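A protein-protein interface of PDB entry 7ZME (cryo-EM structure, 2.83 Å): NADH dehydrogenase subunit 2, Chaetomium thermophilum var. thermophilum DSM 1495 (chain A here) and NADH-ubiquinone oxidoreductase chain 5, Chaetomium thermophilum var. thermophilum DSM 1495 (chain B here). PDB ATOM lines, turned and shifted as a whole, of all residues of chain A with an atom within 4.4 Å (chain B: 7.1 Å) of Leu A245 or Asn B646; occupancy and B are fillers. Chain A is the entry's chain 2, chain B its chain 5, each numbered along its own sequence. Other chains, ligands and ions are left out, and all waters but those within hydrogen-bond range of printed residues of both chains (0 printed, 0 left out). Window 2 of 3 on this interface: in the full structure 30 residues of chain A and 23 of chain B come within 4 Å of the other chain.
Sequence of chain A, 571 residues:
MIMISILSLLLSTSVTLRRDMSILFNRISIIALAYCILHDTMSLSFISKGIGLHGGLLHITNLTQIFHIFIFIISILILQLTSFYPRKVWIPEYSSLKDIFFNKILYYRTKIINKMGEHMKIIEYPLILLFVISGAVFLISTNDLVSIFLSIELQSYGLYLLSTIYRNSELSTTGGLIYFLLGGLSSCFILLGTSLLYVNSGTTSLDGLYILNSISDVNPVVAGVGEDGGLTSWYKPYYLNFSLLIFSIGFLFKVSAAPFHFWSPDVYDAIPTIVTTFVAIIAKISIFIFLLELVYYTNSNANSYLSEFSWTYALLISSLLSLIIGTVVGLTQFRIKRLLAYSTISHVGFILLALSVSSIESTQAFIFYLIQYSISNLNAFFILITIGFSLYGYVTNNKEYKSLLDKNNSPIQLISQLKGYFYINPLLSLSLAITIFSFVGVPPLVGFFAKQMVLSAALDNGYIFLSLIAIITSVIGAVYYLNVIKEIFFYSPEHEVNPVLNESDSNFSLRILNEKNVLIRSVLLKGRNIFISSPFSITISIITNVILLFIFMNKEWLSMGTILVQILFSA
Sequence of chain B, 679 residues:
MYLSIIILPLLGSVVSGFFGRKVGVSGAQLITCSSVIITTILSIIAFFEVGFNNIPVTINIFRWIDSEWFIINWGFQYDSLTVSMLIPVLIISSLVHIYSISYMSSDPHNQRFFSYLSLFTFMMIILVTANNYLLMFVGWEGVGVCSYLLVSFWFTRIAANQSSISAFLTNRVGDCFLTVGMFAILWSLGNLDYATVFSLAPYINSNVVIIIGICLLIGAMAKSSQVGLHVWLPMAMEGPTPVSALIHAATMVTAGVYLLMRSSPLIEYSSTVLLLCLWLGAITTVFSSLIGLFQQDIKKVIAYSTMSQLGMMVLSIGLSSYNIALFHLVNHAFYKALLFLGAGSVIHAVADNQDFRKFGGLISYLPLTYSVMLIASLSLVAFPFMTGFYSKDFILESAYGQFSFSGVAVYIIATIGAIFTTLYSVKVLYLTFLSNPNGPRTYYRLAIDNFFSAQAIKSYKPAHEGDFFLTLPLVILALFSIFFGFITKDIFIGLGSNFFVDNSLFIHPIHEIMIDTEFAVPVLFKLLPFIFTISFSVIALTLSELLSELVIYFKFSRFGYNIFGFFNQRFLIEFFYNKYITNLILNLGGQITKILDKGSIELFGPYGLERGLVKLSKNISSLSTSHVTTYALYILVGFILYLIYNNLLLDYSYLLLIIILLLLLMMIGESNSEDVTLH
OD1 of Asn B646 sits close to O of Phe A309 (3.2 Å).
The backbone carbonyl oxygen of Leu A245 lies within hydrogen-bond range of the side-chain hydroxyl of Ser A248.
Leu A244 touches none of the printed residues of chain B. Leu A245 touches just these residues of chain B: Tyr B642, Leu B643 and Asn B646. Of the printed residues of chain B, Phe A309 touches Asn B646 (3.1 Å), Asn B647 (3.9 Å) and Leu B649 (3.8 Å). Trp A311 touches none of the printed residues of chain B. Printed residues of chain B within 4 Å of Ala A314: Tyr B642. Of the printed residues of chain A, Tyr B642 touches Leu A245 (3.8 Å), Ile A249 (3.7 Å) and Ala A314 (3.5 Å). Printed residues of chain A within 4 Å of Asn B647: Phe A309. The nearest printed residue of chain B that does not touch Leu A245 is Phe B639 (5.9 Å). The nearest residue of chain A that does not touch Asn B646 is Ser A310 (4.1 Å).
Printed residues of chain A that touch a printed residue of chain B: Leu A245, Ile A246, Ile A249, Phe A309 and Ala A314. Hydrophobic or aromatic side chains of chain A that line the printed part of chain B: Leu A245, Ile A246, Ile A249, Phe A309 and Ala A314. Of the 12 printed residues of chain B, 6 touch a printed residue of chain A. Among the printed residues, 10 pairs touch across the chains.
Among the printed residues, pairs that only touch across the chains: Leu A245 with Tyr B642 (3.8 Å), Leu A245 with Leu B643 (3.6 Å), Leu A245 with Asn B646 (3.7 Å), Ile A246 with Phe B639 (3.9 Å), Ile A249 with Phe B639 (3.6 Å), Ile A249 with Tyr B642 (3.7 Å), Phe A309 with Asn B647 (3.9 Å), Phe A309 with Leu B649 (3.8 Å) and Ala A314 with Tyr B642 (3.5 Å).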
ATOM      1  N   ASN A 241      22.368  26.819  -1.091  1.00  0.00           N
ATOM      2  CA  ASN A 241      21.389  26.187  -1.968  1.00  0.00           C
ATOM      3  C   ASN A 241      21.707  24.718  -2.208  1.00  0.00           C
ATOM      4  O   ASN A 241      20.812  23.870  -2.157  1.00  0.00           O
ATOM      5  CB  ASN A 241      21.292  26.932  -3.297  1.00  0.00           C
ATOM      6  CG  ASN A 241      20.375  28.123  -3.227  1.00  0.00           C
ATOM      7  OD1 ASN A 241      19.308  28.062  -2.626  1.00  0.00           O
ATOM      8  ND2 ASN A 241      20.774  29.210  -3.864  1.00  0.00           N
ATOM      9  N   PHE A 242      22.962  24.387  -2.478  1.00  0.00           N
ATOM     10  CA  PHE A 242      23.240  22.989  -2.756  1.00  0.00           C
ATOM     11  C   PHE A 242      23.673  22.168  -1.549  1.00  0.00           C
ATOM     12  O   PHE A 242      23.895  20.966  -1.705  1.00  0.00           O
ATOM     13  CB  PHE A 242      24.226  22.827  -3.931  1.00  0.00           C
ATOM     14  CG  PHE A 242      25.588  23.417  -3.725  1.00  0.00           C
ATOM     15  CD1 PHE A 242      26.592  22.716  -3.123  1.00  0.00           C
ATOM     16  CD2 PHE A 242      25.843  24.706  -4.104  1.00  0.00           C
ATOM     17  CE1 PHE A 242      27.852  23.271  -2.941  1.00  0.00           C
ATOM     18  CE2 PHE A 242      27.100  25.249  -3.943  1.00  0.00           C
ATOM     19  CZ  PHE A 242      28.094  24.538  -3.342  1.00  0.00           C
ATOM     20  N   SER A 243      23.786  22.754  -0.359  1.00  0.00           N
ATOM     21  CA  SER A 243      23.688  21.910   0.828  1.00  0.00           C
ATOM     22  C   SER A 243      22.233  21.605   1.148  1.00  0.00           C
ATOM     23  O   SER A 243      21.909  20.499   1.594  1.00  0.00           O
ATOM     24  CB  SER A 243      24.368  22.566   2.025  1.00  0.00           C
ATOM     25  OG  SER A 243      25.673  22.984   1.689  1.00  0.00           O
ATOM     26  N   LEU A 244      21.344  22.574   0.921  1.00  0.00           N
ATOM     27  CA  LEU A 244      19.920  22.358   1.141  1.00  0.00           C
ATOM     28  C   LEU A 244      19.308  21.437   0.099  1.00  0.00           C
ATOM     29  O   LEU A 244      18.247  20.858   0.352  1.00  0.00           O
ATOM     30  CB  LEU A 244      19.179  23.695   1.154  1.00  0.00           C
ATOM     31  CG  LEU A 244      19.252  24.505   2.451  1.00  0.00           C
ATOM     32  CD1 LEU A 244      18.466  25.791   2.324  1.00  0.00           C
ATOM     33  CD2 LEU A 244      18.760  23.686   3.633  1.00  0.00           C
ATOM     34  N   LEU A 245      19.948  21.294  -1.063  1.00  0.00           N
ATOM     35  CA  LEU A 245      19.461  20.367  -2.078  1.00  0.00           C
ATOM     36  C   LEU A 245      19.685  18.923  -1.654  1.00  0.00           C
ATOM     37  O   LEU A 245      18.790  18.083  -1.778  1.00  0.00           O
ATOM     38  CB  LEU A 245      20.154  20.647  -3.411  1.00  0.00           C
ATOM     39  CG  LEU A 245      19.798  19.739  -4.588  1.00  0.00           C
ATOM     40  CD1 LEU A 245      18.581  20.264  -5.309  1.00  0.00           C
ATOM     41  CD2 LEU A 245      20.965  19.612  -5.538  1.00  0.00           C
ATOM     42  N   ILE A 246      20.887  18.614  -1.164  1.00  0.00           N
ATOM     43  CA  ILE A 246      21.166  17.280  -0.639  1.00  0.00           C
ATOM     44  C   ILE A 246      20.305  17.012   0.585  1.00  0.00           C
ATOM     45  O   ILE A 246      19.773  15.910   0.769  1.00  0.00           O
ATOM     46  CB  ILE A 246      22.666  17.144  -0.324  1.00  0.00           C
ATOM     47  CG1 ILE A 246      23.478  17.176  -1.616  1.00  0.00           C
ATOM     48  CG2 ILE A 246      22.945  15.867   0.446  1.00  0.00           C
ATOM     49  CD1 ILE A 246      24.866  17.702  -1.440  1.00  0.00           C
ATOM     50  N   PHE A 247      20.166  18.018   1.444  1.00  0.00           N
ATOM     51  CA  PHE A 247      19.258  17.946   2.581  1.00  0.00           C
ATOM     52  C   PHE A 247      17.835  17.629   2.136  1.00  0.00           C
ATOM     53  O   PHE A 247      17.156  16.796   2.746  1.00  0.00           O
ATOM     54  CB  PHE A 247      19.330  19.279   3.328  1.00  0.00           C
ATOM     55  CG  PHE A 247      18.589  19.316   4.627  1.00  0.00           C
ATOM     56  CD1 PHE A 247      19.186  18.879   5.791  1.00  0.00           C
ATOM     57  CD2 PHE A 247      17.325  19.872   4.696  1.00  0.00           C
ATOM     58  CE1 PHE A 247      18.516  18.951   6.993  1.00  0.00           C
ATOM     59  CE2 PHE A 247      16.652  19.950   5.894  1.00  0.00           C
ATOM     60  CZ  PHE A 247      17.249  19.488   7.046  1.00  0.00           C
ATOM     61  N   SER A 248      17.374  18.270   1.059  1.00  0.00           N
ATOM     62  CA  SER A 248      16.001  18.083   0.601  1.00  0.00           C
ATOM     63  C   SER A 248      15.786  16.717  -0.037  1.00  0.00           C
ATOM     64  O   SER A 248      14.676  16.176   0.024  1.00  0.00           O
ATOM     65  CB  SER A 248      15.630  19.178  -0.392  1.00  0.00           C
ATOM     66  OG  SER A 248      16.406  19.072  -1.570  1.00  0.00           O
ATOM     67  N   ILE A 249      16.815  16.155  -0.667  1.00  0.00           N
ATOM     68  CA  ILE A 249      16.661  14.864  -1.324  1.00  0.00           C
ATOM     69  C   ILE A 249      16.391  13.772  -0.299  1.00  0.00           C
ATOM     70  O   ILE A 249      15.580  12.866  -0.535  1.00  0.00           O
ATOM     71  CB  ILE A 249      17.903  14.558  -2.183  1.00  0.00           C
ATOM     72  CG1 ILE A 249      17.791  15.268  -3.536  1.00  0.00           C
ATOM     73  CG2 ILE A 249      18.093  13.053  -2.370  1.00  0.00           C
ATOM     74  CD1 ILE A 249      19.040  15.185  -4.370  1.00  0.00           C
ATOM     75  N   PHE A 309      20.055  28.785  -8.651  1.00  0.00           N
ATOM     76  CA  PHE A 309      20.482  27.470  -8.124  1.00  0.00           C
ATOM     77  C   PHE A 309      19.608  27.061  -6.939  1.00  0.00           C
ATOM     78  O   PHE A 309      20.085  26.263  -6.123  1.00  0.00           O
ATOM     79  CB  PHE A 309      21.950  27.552  -7.708  1.00  0.00           C
ATOM     80  CG  PHE A 309      22.915  27.880  -8.818  1.00  0.00           C
ATOM     81  CD1 PHE A 309      23.242  26.936  -9.777  1.00  0.00           C
ATOM     82  CD2 PHE A 309      23.511  29.127  -8.895  1.00  0.00           C
ATOM     83  CE1 PHE A 309      24.132  27.236 -10.795  1.00  0.00           C
ATOM     84  CE2 PHE A 309      24.398  29.429  -9.915  1.00  0.00           C
ATOM     85  CZ  PHE A 309      24.711  28.482 -10.861  1.00  0.00           C
ATOM     86  N   SER A 310      18.363  27.529  -6.877  1.00  0.00           N
ATOM     87  CA  SER A 310      17.530  27.265  -5.680  1.00  0.00           C
ATOM     88  C   SER A 310      17.326  25.772  -5.452  1.00  0.00           C
ATOM     89  O   SER A 310      17.032  25.058  -6.412  1.00  0.00           O
ATOM     90  CB  SER A 310      16.225  27.991  -5.722  1.00  0.00           C
ATOM     91  OG  SER A 310      15.563  27.894  -4.473  1.00  0.00           O
ATOM     92  N   TRP A 311      17.451  25.344  -4.200  1.00  0.00           N
ATOM     93  CA  TRP A 311      17.250  23.927  -3.821  1.00  0.00           C
ATOM     94  C   TRP A 311      15.782  23.580  -4.035  1.00  0.00           C
ATOM     95  O   TRP A 311      15.471  22.389  -4.145  1.00  0.00           O
ATOM     96  CB  TRP A 311      17.654  23.746  -2.362  1.00  0.00           C
ATOM     97  CG  TRP A 311      16.783  24.479  -1.390  1.00  0.00           C
ATOM     98  CD1 TRP A 311      16.852  25.795  -1.040  1.00  0.00           C
ATOM     99  CD2 TRP A 311      15.701  23.917  -0.632  1.00  0.00           C
ATOM    100  NE1 TRP A 311      15.884  26.090  -0.120  1.00  0.00           N
ATOM    101  CE2 TRP A 311      15.165  24.958   0.151  1.00  0.00           C
ATOM    102  CE3 TRP A 311      15.132  22.643  -0.547  1.00  0.00           C
ATOM    103  CZ2 TRP A 311      14.082  24.760   1.001  1.00  0.00           C
ATOM    104  CZ3 TRP A 311      14.067  22.447   0.301  1.00  0.00           C
ATOM    105  CH2 TRP A 311      13.558  23.489   1.072  1.00  0.00           C
ATOM    106  N   ALA A 314      14.417  21.213  -6.883  1.00  0.00           N
ATOM    107  CA  ALA A 314      14.199  19.790  -6.655  1.00  0.00           C
ATOM    108  C   ALA A 314      12.751  19.510  -6.290  1.00  0.00           C
ATOM    109  O   ALA A 314      12.199  18.471  -6.666  1.00  0.00           O
ATOM    110  CB  ALA A 314      15.128  19.291  -5.552  1.00  0.00           C
ATOM    111  N   PHE B 639      19.534  10.913  -7.097  1.00  0.00           N
ATOM    112  CA  PHE B 639      20.297  11.871  -6.306  1.00  0.00           C
ATOM    113  C   PHE B 639      21.296  12.627  -7.171  1.00  0.00           C
ATOM    114  O   PHE B 639      21.327  13.862  -7.170  1.00  0.00           O
ATOM    115  CB  PHE B 639      21.003  11.140  -5.162  1.00  0.00           C
ATOM    116  CG  PHE B 639      22.019  11.974  -4.440  1.00  0.00           C
ATOM    117  CD1 PHE B 639      21.630  12.864  -3.459  1.00  0.00           C
ATOM    118  CD2 PHE B 639      23.367  11.853  -4.731  1.00  0.00           C
ATOM    119  CE1 PHE B 639      22.558  13.623  -2.788  1.00  0.00           C
ATOM    120  CE2 PHE B 639      24.297  12.611  -4.067  1.00  0.00           C
ATOM    121  CZ  PHE B 639      23.892  13.496  -3.092  1.00  0.00           C
ATOM    122  N   ILE B 640      22.117  11.898  -7.928  1.00  0.00           N
ATOM    123  CA  ILE B 640      23.152  12.545  -8.722  1.00  0.00           C
ATOM    124  C   ILE B 640      22.547  13.335  -9.872  1.00  0.00           C
ATOM    125  O   ILE B 640      23.106  14.352 -10.292  1.00  0.00           O
ATOM    126  CB  ILE B 640      24.171  11.505  -9.220  1.00  0.00           C
ATOM    127  CG1 ILE B 640      23.502  10.481 -10.132  1.00  0.00           C
ATOM    128  CG2 ILE B 640      24.822  10.794  -8.056  1.00  0.00           C
ATOM    129  CD1 ILE B 640      24.479   9.582 -10.830  1.00  0.00           C
ATOM    130  N   LEU B 641      21.403  12.890 -10.399  1.00  0.00           N
ATOM    131  CA  LEU B 641      20.753  13.617 -11.485  1.00  0.00           C
ATOM    132  C   LEU B 641      20.262  14.982 -11.020  1.00  0.00           C
ATOM    133  O   LEU B 641      20.321  15.957 -11.778  1.00  0.00           O
ATOM    134  CB  LEU B 641      19.597  12.794 -12.047  1.00  0.00           C
ATOM    135  CG  LEU B 641      19.890  11.950 -13.287  1.00  0.00           C
ATOM    136  CD1 LEU B 641      18.682  11.126 -13.658  1.00  0.00           C
ATOM    137  CD2 LEU B 641      20.328  12.815 -14.452  1.00  0.00           C
ATOM    138  N   TYR B 642      19.761  15.068  -9.786  1.00  0.00           N
ATOM    139  CA  TYR B 642      19.370  16.361  -9.233  1.00  0.00           C
ATOM    140  C   TYR B 642      20.579  17.263  -9.040  1.00  0.00           C
ATOM    141  O   TYR B 642      20.470  18.488  -9.163  1.00  0.00           O
ATOM    142  CB  TYR B 642      18.631  16.172  -7.910  1.00  0.00           C
ATOM    143  CG  TYR B 642      17.158  15.868  -8.049  1.00  0.00           C
ATOM    144  CD1 TYR B 642      16.696  14.987  -9.015  1.00  0.00           C
ATOM    145  CD2 TYR B 642      16.232  16.449  -7.202  1.00  0.00           C
ATOM    146  CE1 TYR B 642      15.349  14.705  -9.136  1.00  0.00           C
ATOM    147  CE2 TYR B 642      14.887  16.170  -7.316  1.00  0.00           C
ATOM    148  CZ  TYR B 642      14.453  15.300  -8.283  1.00  0.00           C
ATOM    149  OH  TYR B 642      13.117  15.021  -8.400  1.00  0.00           O
ATOM    150  N   LEU B 643      21.734  16.680  -8.716  1.00  0.00           N
ATOM    151  CA  LEU B 643      22.962  17.464  -8.658  1.00  0.00           C
ATOM    152  C   LEU B 643      23.354  17.969 -10.041  1.00  0.00           C
ATOM    153  O   LEU B 643      23.807  19.109 -10.184  1.00  0.00           O
ATOM    154  CB  LEU B 643      24.094  16.639  -8.046  1.00  0.00           C
ATOM    155  CG  LEU B 643      23.888  15.922  -6.708  1.00  0.00           C
ATOM    156  CD1 LEU B 643      25.203  15.363  -6.219  1.00  0.00           C
ATOM    157  CD2 LEU B 643      23.299  16.845  -5.665  1.00  0.00           C
ATOM    158  N   ILE B 644      23.200  17.131 -11.069  1.00  0.00           N
ATOM    159  CA  ILE B 644      23.501  17.555 -12.435  1.00  0.00           C
ATOM    160  C   ILE B 644      22.654  18.759 -12.817  1.00  0.00           C
ATOM    161  O   ILE B 644      23.167  19.770 -13.310  1.00  0.00           O
ATOM    162  CB  ILE B 644      23.287  16.396 -13.427  1.00  0.00           C
ATOM    163  CG1 ILE B 644      24.175  15.202 -13.090  1.00  0.00           C
ATOM    164  CG2 ILE B 644      23.528  16.861 -14.852  1.00  0.00           C
ATOM    165  CD1 ILE B 644      25.636  15.505 -13.151  1.00  0.00           C
ATOM    166  N   TYR B 645      21.343  18.668 -12.594  1.00  0.00           N
ATOM    167  CA  TYR B 645      20.449  19.737 -13.022  1.00  0.00           C
ATOM    168  C   TYR B 645      20.759  21.048 -12.319  1.00  0.00           C
ATOM    169  O   TYR B 645      20.724  22.115 -12.940  1.00  0.00           O
ATOM    170  CB  TYR B 645      18.997  19.343 -12.785  1.00  0.00           C
ATOM    171  CG  TYR B 645      18.032  20.351 -13.350  1.00  0.00           C
ATOM    172  CD1 TYR B 645      17.987  20.609 -14.714  1.00  0.00           C
ATOM    173  CD2 TYR B 645      17.200  21.082 -12.520  1.00  0.00           C
ATOM    174  CE1 TYR B 645      17.115  21.543 -15.233  1.00  0.00           C
ATOM    175  CE2 TYR B 645      16.325  22.011 -13.032  1.00  0.00           C
ATOM    176  CZ  TYR B 645      16.288  22.238 -14.388  1.00  0.00           C
ATOM    177  OH  TYR B 645      15.418  23.169 -14.896  1.00  0.00           O
ATOM    178  N   ASN B 646      21.064  20.991 -11.025  1.00  0.00           N
ATOM    179  CA  ASN B 646      21.230  22.220 -10.264  1.00  0.00           C
ATOM    180  C   ASN B 646      22.625  22.807 -10.453  1.00  0.00           C
ATOM    181  O   ASN B 646      22.769  23.992 -10.769  1.00  0.00           O
ATOM    182  CB  ASN B 646      20.948  21.954  -8.785  1.00  0.00           C
ATOM    183  CG  ASN B 646      20.835  23.229  -7.978  1.00  0.00           C
ATOM    184  OD1 ASN B 646      20.974  24.327  -8.512  1.00  0.00           O
ATOM    185  ND2 ASN B 646      20.581  23.092  -6.683  1.00  0.00           N
ATOM    186  N   ASN B 647      23.662  21.989 -10.266  1.00  0.00           N
ATOM    187  CA  ASN B 647      25.029  22.496 -10.314  1.00  0.00           C
ATOM    188  C   ASN B 647      25.402  22.982 -11.709  1.00  0.00           C
ATOM    189  O   ASN B 647      26.047  24.027 -11.856  1.00  0.00           O
ATOM    190  CB  ASN B 647      26.002  21.417  -9.845  1.00  0.00           C
ATOM    191  CG  ASN B 647      27.348  21.980  -9.439  1.00  0.00           C
ATOM    192  OD1 ASN B 647      27.637  23.156  -9.661  1.00  0.00           O
ATOM    193  ND2 ASN B 647      28.178  21.141  -8.833  1.00  0.00           N
ATOM    194  N   LEU B 648      25.008  22.244 -12.745  1.00  0.00           N
ATOM    195  CA  LEU B 648      25.424  22.582 -14.099  1.00  0.00           C
ATOM    196  C   LEU B 648      24.613  23.711 -14.717  1.00  0.00           C
ATOM    197  O   LEU B 648      24.958  24.161 -15.815  1.00  0.00           O
ATOM    198  CB  LEU B 648      25.345  21.349 -15.000  1.00  0.00           C
ATOM    199  CG  LEU B 648      26.437  20.300 -14.790  1.00  0.00           C
ATOM    200  CD1 LEU B 648      26.253  19.134 -15.749  1.00  0.00           C
ATOM    201  CD2 LEU B 648      27.812  20.924 -14.956  1.00  0.00           C
ATOM    202  N   LEU B 649      23.562  24.180 -14.043  1.00  0.00           N
ATOM    203  CA  LEU B 649      22.720  25.267 -14.544  1.00  0.00           C
ATOM    204  C   LEU B 649      22.181  24.941 -15.936  1.00  0.00           C
ATOM    205  O   LEU B 649      22.216  25.759 -16.859  1.00  0.00           O
ATOM    206  CB  LEU B 649      23.482  26.595 -14.540  1.00  0.00           C
ATOM    207  CG  LEU B 649      22.654  27.881 -14.608  1.00  0.00           C
ATOM    208  CD1 LEU B 649      21.503  27.837 -13.615  1.00  0.00           C
ATOM    209  CD2 LEU B 649      23.531  29.101 -14.370  1.00  0.00           C
ATOM    210  N   LEU B 650      21.692  23.715 -16.084  1.00  0.00           N
ATOM    211  CA  LEU B 650      21.137  23.276 -17.354  1.00  0.00           C
ATOM    212  C   LEU B 650      19.880  24.070 -17.695  1.00  0.00           C
ATOM    213  O   LEU B 650      19.231  24.666 -16.830  1.00  0.00           O
ATOM    214  CB  LEU B 650      20.807  21.785 -17.307  1.00  0.00           C
ATOM    215  CG  LEU B 650      21.922  20.838 -16.867  1.00  0.00           C
ATOM    216  CD1 LEU B 650      21.398  19.416 -16.767  1.00  0.00           C
ATOM    217  CD2 LEU B 650      23.091  20.911 -17.835  1.00  0.00           C
